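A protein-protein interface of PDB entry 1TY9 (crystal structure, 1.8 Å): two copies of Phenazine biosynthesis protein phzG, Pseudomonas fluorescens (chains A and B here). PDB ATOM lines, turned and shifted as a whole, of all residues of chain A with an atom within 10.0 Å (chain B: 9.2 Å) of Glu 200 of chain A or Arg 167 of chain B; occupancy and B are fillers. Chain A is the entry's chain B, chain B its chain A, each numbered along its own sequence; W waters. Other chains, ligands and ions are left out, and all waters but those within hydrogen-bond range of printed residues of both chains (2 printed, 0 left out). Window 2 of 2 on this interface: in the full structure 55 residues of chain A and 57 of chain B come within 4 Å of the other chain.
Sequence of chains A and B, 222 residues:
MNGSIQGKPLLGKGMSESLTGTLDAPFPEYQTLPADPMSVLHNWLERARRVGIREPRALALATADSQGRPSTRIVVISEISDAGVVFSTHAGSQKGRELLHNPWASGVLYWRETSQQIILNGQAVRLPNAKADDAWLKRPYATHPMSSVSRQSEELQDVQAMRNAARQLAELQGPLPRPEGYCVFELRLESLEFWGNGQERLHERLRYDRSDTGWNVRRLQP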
ATOM      1  N   GLY A 196       7.464  25.321  17.579  1.00  0.00           N
ATOM      2  CA  GLY A 196       8.907  25.159  17.863  1.00  0.00           C
ATOM      3  C   GLY A 196       9.648  24.478  16.735  1.00  0.00           C
ATOM      4  O   GLY A 196       9.077  23.755  15.915  1.00  0.00           O
ATOM      5  N   ASN A 197      10.951  24.679  16.673  1.00  0.00           N
ATOM      6  CA  ASN A 197      11.723  24.073  15.591  1.00  0.00           C
ATOM      7  C   ASN A 197      11.700  22.519  15.591  1.00  0.00           C
ATOM      8  O   ASN A 197      11.767  21.919  14.519  1.00  0.00           O
ATOM      9  CB  ASN A 197      13.180  24.582  15.652  1.00  0.00           C
ATOM     10  CG  ASN A 197      13.913  24.336  14.366  1.00  0.00           C
ATOM     11  OD1 ASN A 197      13.410  24.640  13.268  1.00  0.00           O
ATOM     12  ND2 ASN A 197      15.115  23.755  14.484  1.00  0.00           N
ATOM     13  N   GLY A 198      11.517  21.899  16.759  1.00  0.00           N
ATOM     14  CA  GLY A 198      11.415  20.415  16.864  1.00  0.00           C
ATOM     15  C   GLY A 198      12.760  19.718  16.567  1.00  0.00           C
ATOM     16  O   GLY A 198      13.806  20.357  16.571  1.00  0.00           O
ATOM     17  N   GLN A 199      12.708  18.427  16.252  1.00  0.00           N
ATOM     18  CA  GLN A 199      13.935  17.684  15.896  1.00  0.00           C
ATOM     19  C   GLN A 199      13.766  17.109  14.523  1.00  0.00           C
ATOM     20  O   GLN A 199      12.652  16.750  14.124  1.00  0.00           O
ATOM     21  CB  GLN A 199      14.260  16.576  16.938  1.00  0.00           C
ATOM     22  CG  GLN A 199      14.507  17.092  18.433  1.00  0.00           C
ATOM     23  CD  GLN A 199      13.193  17.487  19.201  1.00  0.00           C
ATOM     24  OE1 GLN A 199      13.103  18.558  19.886  1.00  0.00           O
ATOM     25  NE2 GLN A 199      12.185  16.618  19.101  1.00  0.00           N
ATOM     26  N   GLU A 200      14.881  17.066  13.766  1.00  0.00           N
ATOM     27  CA  GLU A 200      14.894  16.534  12.419  1.00  0.00           C
ATOM     28  C   GLU A 200      13.882  17.190  11.492  1.00  0.00           C
ATOM     29  O   GLU A 200      13.306  16.522  10.582  1.00  0.00           O
ATOM     30  CB  GLU A 200      14.659  15.022  12.454  1.00  0.00           C
ATOM     31  CG  GLU A 200      15.522  14.308  13.460  1.00  0.00           C
ATOM     32  CD  GLU A 200      15.350  12.796  13.447  1.00  0.00           C
ATOM     33  OE1 GLU A 200      14.208  12.275  13.401  1.00  0.00           O
ATOM     34  OE2 GLU A 200      16.403  12.112  13.534  1.00  0.00           O
ATOM     35  N   ARG A 201      13.668  18.487  11.728  1.00  0.00           N
ATOM     36  CA  ARG A 201      12.788  19.318  10.922  1.00  0.00           C
ATOM     37  C   ARG A 201      11.321  18.935  11.072  1.00  0.00           C
ATOM     38  O   ARG A 201      10.476  19.514  10.378  1.00  0.00           O
ATOM     39  CB  ARG A 201      13.229  19.248   9.437  1.00  0.00           C
ATOM     40  CG  ARG A 201      14.757  19.605   9.191  1.00  0.00           C
ATOM     41  CD  ARG A 201      15.053  20.099   7.762  1.00  0.00           C
ATOM     42  NE  ARG A 201      16.016  21.218   7.672  1.00  0.00           N
ATOM     43  CZ  ARG A 201      17.348  21.097   7.806  1.00  0.00           C
ATOM     44  NH1 ARG A 201      17.900  19.930   8.120  1.00  0.00           N
ATOM     45  NH2 ARG A 201      18.128  22.172   7.686  1.00  0.00           N
ATOM     46  N   LEU A 202      11.008  18.039  12.030  1.00  0.00           N
ATOM     47  CA  LEU A 202       9.632  17.820  12.418  1.00  0.00           C
ATOM     48  C   LEU A 202       9.206  18.971  13.325  1.00  0.00           C
ATOM     49  O   LEU A 202       9.086  18.809  14.537  1.00  0.00           O
ATOM     50  CB  LEU A 202       9.432  16.443  13.121  1.00  0.00           C
ATOM     51  CG  LEU A 202       8.009  15.829  12.865  1.00  0.00           C
ATOM     52  CD1 LEU A 202       7.899  14.367  13.315  1.00  0.00           C
ATOM     53  CD2 LEU A 202       6.917  16.642  13.565  1.00  0.00           C
ATOM     54  N   HIS A 203       8.873  20.099  12.723  1.00  0.00           N
ATOM     55  CA  HIS A 203       8.498  21.260  13.491  1.00  0.00           C
ATOM     56  C   HIS A 203       7.275  21.002  14.313  1.00  0.00           C
ATOM     57  O   HIS A 203       6.302  20.364  13.858  1.00  0.00           O
ATOM     58  CB  HIS A 203       8.288  22.491  12.612  1.00  0.00           C
ATOM     59  CG  HIS A 203       9.411  22.720  11.660  1.00  0.00           C
ATOM     60  ND1 HIS A 203      10.739  22.771  12.062  1.00  0.00           N
ATOM     61  CD2 HIS A 203       9.405  22.947  10.334  1.00  0.00           C
ATOM     62  CE1 HIS A 203      11.500  22.967  10.997  1.00  0.00           C
ATOM     63  NE2 HIS A 203      10.711  23.042   9.937  1.00  0.00           N
ATOM     64  N   GLU A 204       7.359  21.468  15.543  1.00  0.00           N
ATOM     65  CA  GLU A 204       6.332  21.169  16.575  1.00  0.00           C
ATOM     66  C   GLU A 204       5.278  22.238  16.608  1.00  0.00           C
ATOM     67  O   GLU A 204       5.525  23.382  17.054  1.00  0.00           O
ATOM     68  CB  GLU A 204       6.962  20.955  17.948  1.00  0.00           C
ATOM     69  CG  GLU A 204       7.804  19.691  17.823  1.00  0.00           C
ATOM     70  CD  GLU A 204       8.774  19.389  18.971  1.00  0.00           C
ATOM     71  OE1 GLU A 204       8.920  20.174  19.921  1.00  0.00           O
ATOM     72  OE2 GLU A 204       9.374  18.311  18.883  1.00  0.00           O
ATOM     73  N   PRO A 222       4.056  19.849   9.886  1.00  0.00           N
ATOM     74  CA  PRO A 222       5.016  20.928   9.628  1.00  0.00           C
ATOM     75  C   PRO A 222       4.987  21.405   8.170  1.00  0.00           C
ATOM     76  O   PRO A 222       5.262  22.549   7.915  1.00  0.00           O
ATOM     77  CB  PRO A 222       6.374  20.305   9.988  1.00  0.00           C
ATOM     78  CG  PRO A 222       6.193  18.851   9.953  1.00  0.00           C
ATOM     79  CD  PRO A 222       4.698  18.543  10.147  1.00  0.00           C
ATOM     80  OXT PRO A 222       4.706  20.662   7.204  1.00  0.00           O
ATOM     81  N   ALA B 142      18.781  18.244   2.860  1.00  0.00           N
ATOM     82  CA  ALA B 142      18.293  17.765   4.183  1.00  0.00           C
ATOM     83  C   ALA B 142      16.843  18.165   4.460  1.00  0.00           C
ATOM     84  O   ALA B 142      16.182  17.568   5.363  1.00  0.00           O
ATOM     85  CB  ALA B 142      19.170  18.287   5.331  1.00  0.00           C
ATOM     86  N   THR B 143      16.356  19.174   3.726  1.00  0.00           N
ATOM     87  CA  THR B 143      14.962  19.608   3.876  1.00  0.00           C
ATOM     88  C   THR B 143      13.974  18.773   3.068  1.00  0.00           C
ATOM     89  O   THR B 143      12.798  18.875   3.313  1.00  0.00           O
ATOM     90  CB  THR B 143      14.742  21.103   3.532  1.00  0.00           C
ATOM     91  OG1 THR B 143      14.985  21.305   2.138  1.00  0.00           O
ATOM     92  CG2 THR B 143      15.800  22.038   4.288  1.00  0.00           C
ATOM     93  N   HIS B 144      14.423  17.958   2.116  1.00  0.00           N
ATOM     94  CA  HIS B 144      13.458  17.232   1.284  1.00  0.00           C
ATOM     95  C   HIS B 144      12.589  16.193   2.020  1.00  0.00           C
ATOM     96  O   HIS B 144      11.374  16.097   1.755  1.00  0.00           O
ATOM     97  CB  HIS B 144      14.216  16.615   0.067  1.00  0.00           C
ATOM     98  CG  HIS B 144      14.667  17.654  -0.912  1.00  0.00           C
ATOM     99  ND1 HIS B 144      15.173  17.329  -2.145  1.00  0.00           N
ATOM    100  CD2 HIS B 144      14.641  19.017  -0.856  1.00  0.00           C
ATOM    101  CE1 HIS B 144      15.450  18.439  -2.811  1.00  0.00           C
ATOM    102  NE2 HIS B 144      15.133  19.477  -2.056  1.00  0.00           N
ATOM    103  N   PRO B 145      13.201  15.353   2.874  1.00  0.00           N
ATOM    104  CA  PRO B 145      12.441  14.273   3.533  1.00  0.00           C
ATOM    105  C   PRO B 145      11.165  14.745   4.254  1.00  0.00           C
ATOM    106  O   PRO B 145      10.061  14.232   3.986  1.00  0.00           O
ATOM    107  CB  PRO B 145      13.463  13.678   4.510  1.00  0.00           C
ATOM    108  CG  PRO B 145      14.807  13.913   3.778  1.00  0.00           C
ATOM    109  CD  PRO B 145      14.653  15.295   3.217  1.00  0.00           C
ATOM    110  N   MET B 146      11.305  15.740   5.134  1.00  0.00           N
ATOM    111  CA  MET B 146      10.167  16.093   5.948  1.00  0.00           C
ATOM    112  C   MET B 146       9.139  16.848   5.100  1.00  0.00           C
ATOM    113  O   MET B 146       7.948  16.555   5.198  1.00  0.00           O
ATOM    114  CB  MET B 146      10.573  16.916   7.175  1.00  0.00           C
ATOM    115  CG  MET B 146       9.434  17.057   8.218  1.00  0.00           C
ATOM    116  SD  MET B 146       9.007  15.472   9.018  1.00  0.00           S
ATOM    117  CE  MET B 146      10.488  15.054   9.870  1.00  0.00           C
ATOM    118  N   SER B 147       9.607  17.795   4.269  1.00  0.00           N
ATOM    119  CA  SER B 147       8.715  18.526   3.394  1.00  0.00           C
ATOM    120  C   SER B 147       8.019  17.594   2.403  1.00  0.00           C
ATOM    121  O   SER B 147       6.973  17.965   1.879  1.00  0.00           O
ATOM    122  CB  SER B 147       9.441  19.646   2.611  1.00  0.00           C
ATOM    123  OG  SER B 147      10.106  20.533   3.493  1.00  0.00           O
ATOM    124  N   VAL B 149       7.208  14.259   3.245  1.00  0.00           N
ATOM    125  CA  VAL B 149       6.258  13.400   4.000  1.00  0.00           C
ATOM    126  C   VAL B 149       5.057  14.217   4.600  1.00  0.00           C
ATOM    127  O   VAL B 149       3.913  13.736   4.664  1.00  0.00           O
ATOM    128  CB  VAL B 149       6.995  12.571   5.036  1.00  0.00           C
ATOM    129  CG1 VAL B 149       8.064  11.654   4.382  1.00  0.00           C
ATOM    130  CG2 VAL B 149       7.655  13.508   6.007  1.00  0.00           C
ATOM    131  N   VAL B 159       2.791  11.310  15.433  1.00  0.00           N
ATOM    132  CA  VAL B 159       4.085  12.015  15.368  1.00  0.00           C
ATOM    133  C   VAL B 159       5.181  11.049  14.954  1.00  0.00           C
ATOM    134  O   VAL B 159       5.966  11.310  13.993  1.00  0.00           O
ATOM    135  CB  VAL B 159       4.434  12.663  16.696  1.00  0.00           C
ATOM    136  CG1 VAL B 159       5.797  13.292  16.610  1.00  0.00           C
ATOM    137  CG2 VAL B 159       3.391  13.725  17.044  1.00  0.00           C
ATOM    138  N   GLN B 160       5.194   9.912  15.633  1.00  0.00           N
ATOM    139  CA  GLN B 160       6.247   8.932  15.398  1.00  0.00           C
ATOM    140  C   GLN B 160       6.216   8.370  13.957  1.00  0.00           C
ATOM    141  O   GLN B 160       7.281   8.183  13.344  1.00  0.00           O
ATOM    142  CB  GLN B 160       6.201   7.794  16.408  1.00  0.00           C
ATOM    143  CG  GLN B 160       7.444   6.896  16.279  1.00  0.00           C
ATOM    144  CD  GLN B 160       8.727   7.590  16.720  1.00  0.00           C
ATOM    145  OE1 GLN B 160       9.792   7.468  16.071  1.00  0.00           O
ATOM    146  NE2 GLN B 160       8.646   8.314  17.849  1.00  0.00           N
ATOM    147  N   ALA B 161       5.023   8.162  13.423  1.00  0.00           N
ATOM    148  CA  ALA B 161       4.892   7.683  12.056  1.00  0.00           C
ATOM    149  C   ALA B 161       5.517   8.685  11.078  1.00  0.00           C
ATOM    150  O   ALA B 161       6.254   8.302  10.160  1.00  0.00           O
ATOM    151  CB  ALA B 161       3.447   7.385  11.678  1.00  0.00           C
ATOM    152  N   MET B 162       5.218   9.961  11.267  1.00  0.00           N
ATOM    153  CA  MET B 162       5.837  10.975  10.450  1.00  0.00           C
ATOM    154  C   MET B 162       7.356  10.945  10.620  1.00  0.00           C
ATOM    155  O   MET B 162       8.086  11.020   9.645  1.00  0.00           O
ATOM    156  CB  MET B 162       5.287  12.379  10.801  1.00  0.00           C
ATOM    157  CG  MET B 162       6.034  13.429   9.981  1.00  0.00           C
ATOM    158  SD  MET B 162       5.286  15.056  10.138  1.00  0.00           S
ATOM    159  CE  MET B 162       3.843  14.738   9.162  1.00  0.00           C
ATOM    160  N   ARG B 163       7.851  10.809  11.850  1.00  0.00           N
ATOM    161  CA  ARG B 163       9.280  10.864  12.037  1.00  0.00           C
ATOM    162  C   ARG B 163       9.957   9.679  11.307  1.00  0.00           C
ATOM    163  O   ARG B 163      11.004   9.849  10.657  1.00  0.00           O
ATOM    164  CB  ARG B 163       9.593  10.880  13.544  1.00  0.00           C
ATOM    165  CG  ARG B 163      11.036  11.025  13.918  1.00  0.00           C
ATOM    166  CD  ARG B 163      11.316  11.282  15.454  1.00  0.00           C
ATOM    167  NE  ARG B 163      10.498  12.322  16.084  1.00  0.00           N
ATOM    168  CZ  ARG B 163      10.665  13.656  15.934  1.00  0.00           C
ATOM    169  NH1 ARG B 163      11.611  14.164  15.113  1.00  0.00           N
ATOM    170  NH2 ARG B 163       9.829  14.466  16.566  1.00  0.00           N
ATOM    171  N   ASN B 164       9.350   8.512  11.431  1.00  0.00           N
ATOM    172  CA  ASN B 164       9.890   7.272  10.845  1.00  0.00           C
ATOM    173  C   ASN B 164       9.919   7.310   9.308  1.00  0.00           C
ATOM    174  O   ASN B 164      10.913   6.929   8.712  1.00  0.00           O
ATOM    175  CB  ASN B 164       9.096   6.077  11.357  1.00  0.00           C
ATOM    176  CG  ASN B 164       9.458   5.689  12.798  1.00  0.00           C
ATOM    177  OD1 ASN B 164       8.839   4.826  13.375  1.00  0.00           O
ATOM    178  ND2 ASN B 164      10.424   6.326  13.353  1.00  0.00           N
ATOM    179  N   ALA B 165       8.834   7.810   8.697  1.00  0.00           N
ATOM    180  CA  ALA B 165       8.697   7.865   7.260  1.00  0.00           C
ATOM    181  C   ALA B 165       9.739   8.871   6.750  1.00  0.00           C
ATOM    182  O   ALA B 165      10.375   8.619   5.745  1.00  0.00           O
ATOM    183  CB  ALA B 165       7.234   8.272   6.863  1.00  0.00           C
ATOM    184  N   ALA B 166       9.926  10.004   7.448  1.00  0.00           N
ATOM    185  CA  ALA B 166      10.938  10.987   7.026  1.00  0.00           C
ATOM    186  C   ALA B 166      12.356  10.400   7.120  1.00  0.00           C
ATOM    187  O   ALA B 166      13.169  10.626   6.247  1.00  0.00           O
ATOM    188  CB  ALA B 166      10.816  12.277   7.814  1.00  0.00           C
ATOM    189  N   ARG B 167      12.628   9.628   8.181  1.00  0.00           N
ATOM    190  CA  ARG B 167      13.972   8.994   8.372  1.00  0.00           C
ATOM    191  C   ARG B 167      14.312   8.083   7.188  1.00  0.00           C
ATOM    192  O   ARG B 167      15.481   8.066   6.727  1.00  0.00           O
ATOM    193  CB  ARG B 167      14.081   8.224   9.704  1.00  0.00           C
ATOM    194  CG  ARG B 167      14.234   9.172  10.932  1.00  0.00           C
ATOM    195  CD  ARG B 167      14.157   8.486  12.270  1.00  0.00           C
ATOM    196  NE  ARG B 167      14.429   9.419  13.373  1.00  0.00           N
ATOM    197  CZ  ARG B 167      14.266   9.111  14.667  1.00  0.00           C
ATOM    198  NH1 ARG B 167      13.834   7.898  14.994  1.00  0.00           N
ATOM    199  NH2 ARG B 167      14.537   9.995  15.636  1.00  0.00           N
ATOM    200  N   GLN B 168      13.314   7.318   6.735  1.00  0.00           N
ATOM    201  CA  GLN B 168      13.383   6.525   5.481  1.00  0.00           C
ATOM    202  C   GLN B 168      13.882   7.355   4.280  1.00  0.00           C
ATOM    203  O   GLN B 168      14.845   6.963   3.586  1.00  0.00           O
ATOM    204  CB  GLN B 168      12.021   5.886   5.158  1.00  0.00           C
ATOM    205  CG  GLN B 168      11.719   4.591   5.893  1.00  0.00           C
ATOM    206  CD  GLN B 168      12.597   3.373   5.442  1.00  0.00           C
ATOM    207  OE1 GLN B 168      13.219   3.412   4.385  1.00  0.00           O
ATOM    208  NE2 GLN B 168      12.635   2.314   6.245  1.00  0.00           N
ATOM    209  N   LEU B 169      13.292   8.527   4.043  1.00  0.00           N
ATOM    210  CA  LEU B 169      13.802   9.360   2.962  1.00  0.00           C
ATOM    211  C   LEU B 169      15.136  10.089   3.273  1.00  0.00           C
ATOM    212  O   LEU B 169      15.928  10.327   2.332  1.00  0.00           O
ATOM    213  CB  LEU B 169      12.712  10.327   2.435  1.00  0.00           C
ATOM    214  CG  LEU B 169      11.343   9.773   2.072  1.00  0.00           C
ATOM    215  CD1 LEU B 169      10.414  10.955   1.769  1.00  0.00           C
ATOM    216  CD2 LEU B 169      11.376   8.843   0.844  1.00  0.00           C
ATOM    217  N   ALA B 170      15.425  10.398   4.552  1.00  0.00           N
ATOM    218  CA  ALA B 170      16.669  11.077   4.956  1.00  0.00           C
ATOM    219  C   ALA B 170      17.909  10.288   4.577  1.00  0.00           C
ATOM    220  O   ALA B 170      18.986  10.859   4.308  1.00  0.00           O
ATOM    221  CB  ALA B 170      16.683  11.401   6.469  1.00  0.00           C
ATOM    222  N   GLU B 171      17.723   8.980   4.515  1.00  0.00           N
ATOM    223  CA  GLU B 171      18.809   8.046   4.300  1.00  0.00           C
ATOM    224  C   GLU B 171      19.289   8.091   2.861  1.00  0.00           C
ATOM    225  O   GLU B 171      20.428   7.696   2.575  1.00  0.00           O
ATOM    226  CB  GLU B 171      18.311   6.625   4.590  1.00  0.00           C
ATOM    227  CG  GLU B 171      18.734   6.088   5.946  1.00  0.00           C
ATOM    228  CD  GLU B 171      17.888   4.907   6.397  1.00  0.00           C
ATOM    229  OE1 GLU B 171      17.525   4.039   5.571  1.00  0.00           O
ATOM    230  OE2 GLU B 171      17.575   4.871   7.610  1.00  0.00           O
ATOM    231  N   LEU B 172      18.420   8.554   1.952  1.00  0.00           N
ATOM    232  CA  LEU B 172      18.727   8.546   0.517  1.00  0.00           C
ATOM    233  C   LEU B 172      19.760   9.608   0.164  1.00  0.00           C
ATOM    234  O   LEU B 172      19.956  10.542   0.920  1.00  0.00           O
ATOM    235  CB  LEU B 172      17.454   8.753  -0.272  1.00  0.00           C
ATOM    236  CG  LEU B 172      16.566   7.506  -0.401  1.00  0.00           C
ATOM    237  CD1 LEU B 172      16.582   6.640   0.860  1.00  0.00           C
ATOM    238  CD2 LEU B 172      15.157   7.915  -0.779  1.00  0.00           C
ATOM    239  N   LEU B 176      15.398  14.817  -3.602  1.00  0.00           N
ATOM    240  CA  LEU B 176      14.207  14.063  -3.839  1.00  0.00           C
ATOM    241  C   LEU B 176      13.379  14.772  -4.917  1.00  0.00           C
ATOM    242  O   LEU B 176      13.638  15.933  -5.216  1.00  0.00           O
ATOM    243  CB  LEU B 176      13.440  13.947  -2.523  1.00  0.00           C
ATOM    244  CG  LEU B 176      14.136  13.257  -1.330  1.00  0.00           C
ATOM    245  CD1 LEU B 176      13.165  13.133  -0.129  1.00  0.00           C
ATOM    246  CD2 LEU B 176      14.801  11.863  -1.667  1.00  0.00           C
HETATM  247  O   HOH W   1      12.583  12.243  11.158  1.00  0.00           O
HETATM  248  O   HOH W   2      10.122  17.394  16.682  1.00  0.00           O
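O of Glu 200 of chain A touches CE of Met 146 of chain B, 3.3 Å away.
Ala 142 of chain B touches Arg 201 of chain A (CB to NH1, 3.5 Å).
CG2 of Thr 143 of chain B touches NE of Arg 201 of chain A, at 3.5 Å.
Arg 201 of chain A touches Met 146 of chain B.
CB of Leu 202 of chain A touches CE of Met 146 of chain B (3.7 Å).
CD1 of Leu 202 of chain A touches O of Val 159 of chain B, at 3.7 Å.
Met 162 of chain B touches Leu 202 of chain A.
Leu 202 of chain A touches Arg 163 of chain B.
Met 162 of chain B touches Pro 222 of chain A.
Of the printed residues of chain B, Glu 200 of chain A touches Met 146, Arg 163 and Arg 167.
Of chain A, only Glu 200 (2.9 Å) comes within 4 Å of Arg 167 of chain B.
No residue of chain A comes within 4 Å of Ala 165 of chain B.
Ala 166 of chain B touches none of the printed residues of chain A.
Of the printed residues of chain B, Pro 222 of chain A touches Met 162 (3.5 Å).
Of the printed residues of chain B, Leu 202 of chain A touches Met 146, Val 159, Met 162 and Arg 163.
Printed residues of chain B within 4 Å of Arg 201 of chain A: Ala 142 (3.5 Å), Thr 143 (3.5 Å) and Met 146 (3.4 Å).
Gln 168 of chain B touches none of the printed residues of chain A.
Gly 196 of chain A touches none of the printed residues of chain B.
The nearest residue of chain A that does not touch Arg 167 of chain B is Gln 199 of chain A (6.7 Å).
No position is printed for both chains.
The guanidinium group (NE) of Arg 167 of chain B lies within salt-bridge range of the side-chain carboxylate (OE1) of Glu 200 of chain A, at 2.9 Å.
The backbone carbonyl oxygen (O) of Gln 199 of chain A is in hydrogen-bond range of the guanidinium group (NH1) of Arg 163 of chain B.
The guanidinium group (NH1) of Arg 163 of chain B is in salt-bridge range of the side-chain carboxylate (OE1) of Glu 200 of chain A, at 3.6 Å.
Water W2 lies within hydrogen-bond range of OE2 of Glu 204 of chain A, O of Leu 202 of chain A, N of Gln 199 of chain A and NH2 of Arg 163 of chain B.
Water W1 lies within hydrogen-bond range of the side-chain carboxylate (OE1) of Glu 200 of chain A (2.8 Å) and the backbone carbonyl oxygen (O) of Arg 163 of chain B (2.9 Å).
The side-chain amide nitrogen (NE2) of Gln 199 of chain A lies within hydrogen-bond range of the side-chain carboxylate (OE2) of Glu 204 of chain A (3.3 Å).
The backbone carbonyl oxygen of Thr 143 of chain B lies within hydrogen-bond range of the side-chain hydroxyl of Ser 147 of chain B, at 3.2 Å.
Of the 22 printed residues of chain B, 7 touch a printed residue of chain A.
Hydrophobic or aromatic side chains of chain B that line the printed part of chain A: Ala 142, Met 146 and Met 162.
Printed residues of chain A that touch a printed residue of chain B: Gln 199, Glu 200, Arg 201, Leu 202 and Pro 222.
Among the printed residues, 12 pairs touch across the chains.
Among the printed residues, Asp or Glu carboxylates within 4 Å of a Lys or Arg side-chain nitrogen of the other chain: Glu 200 of chain A with Arg 163 of chain B and Glu 200 of chain A with Arg 167 of chain B.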
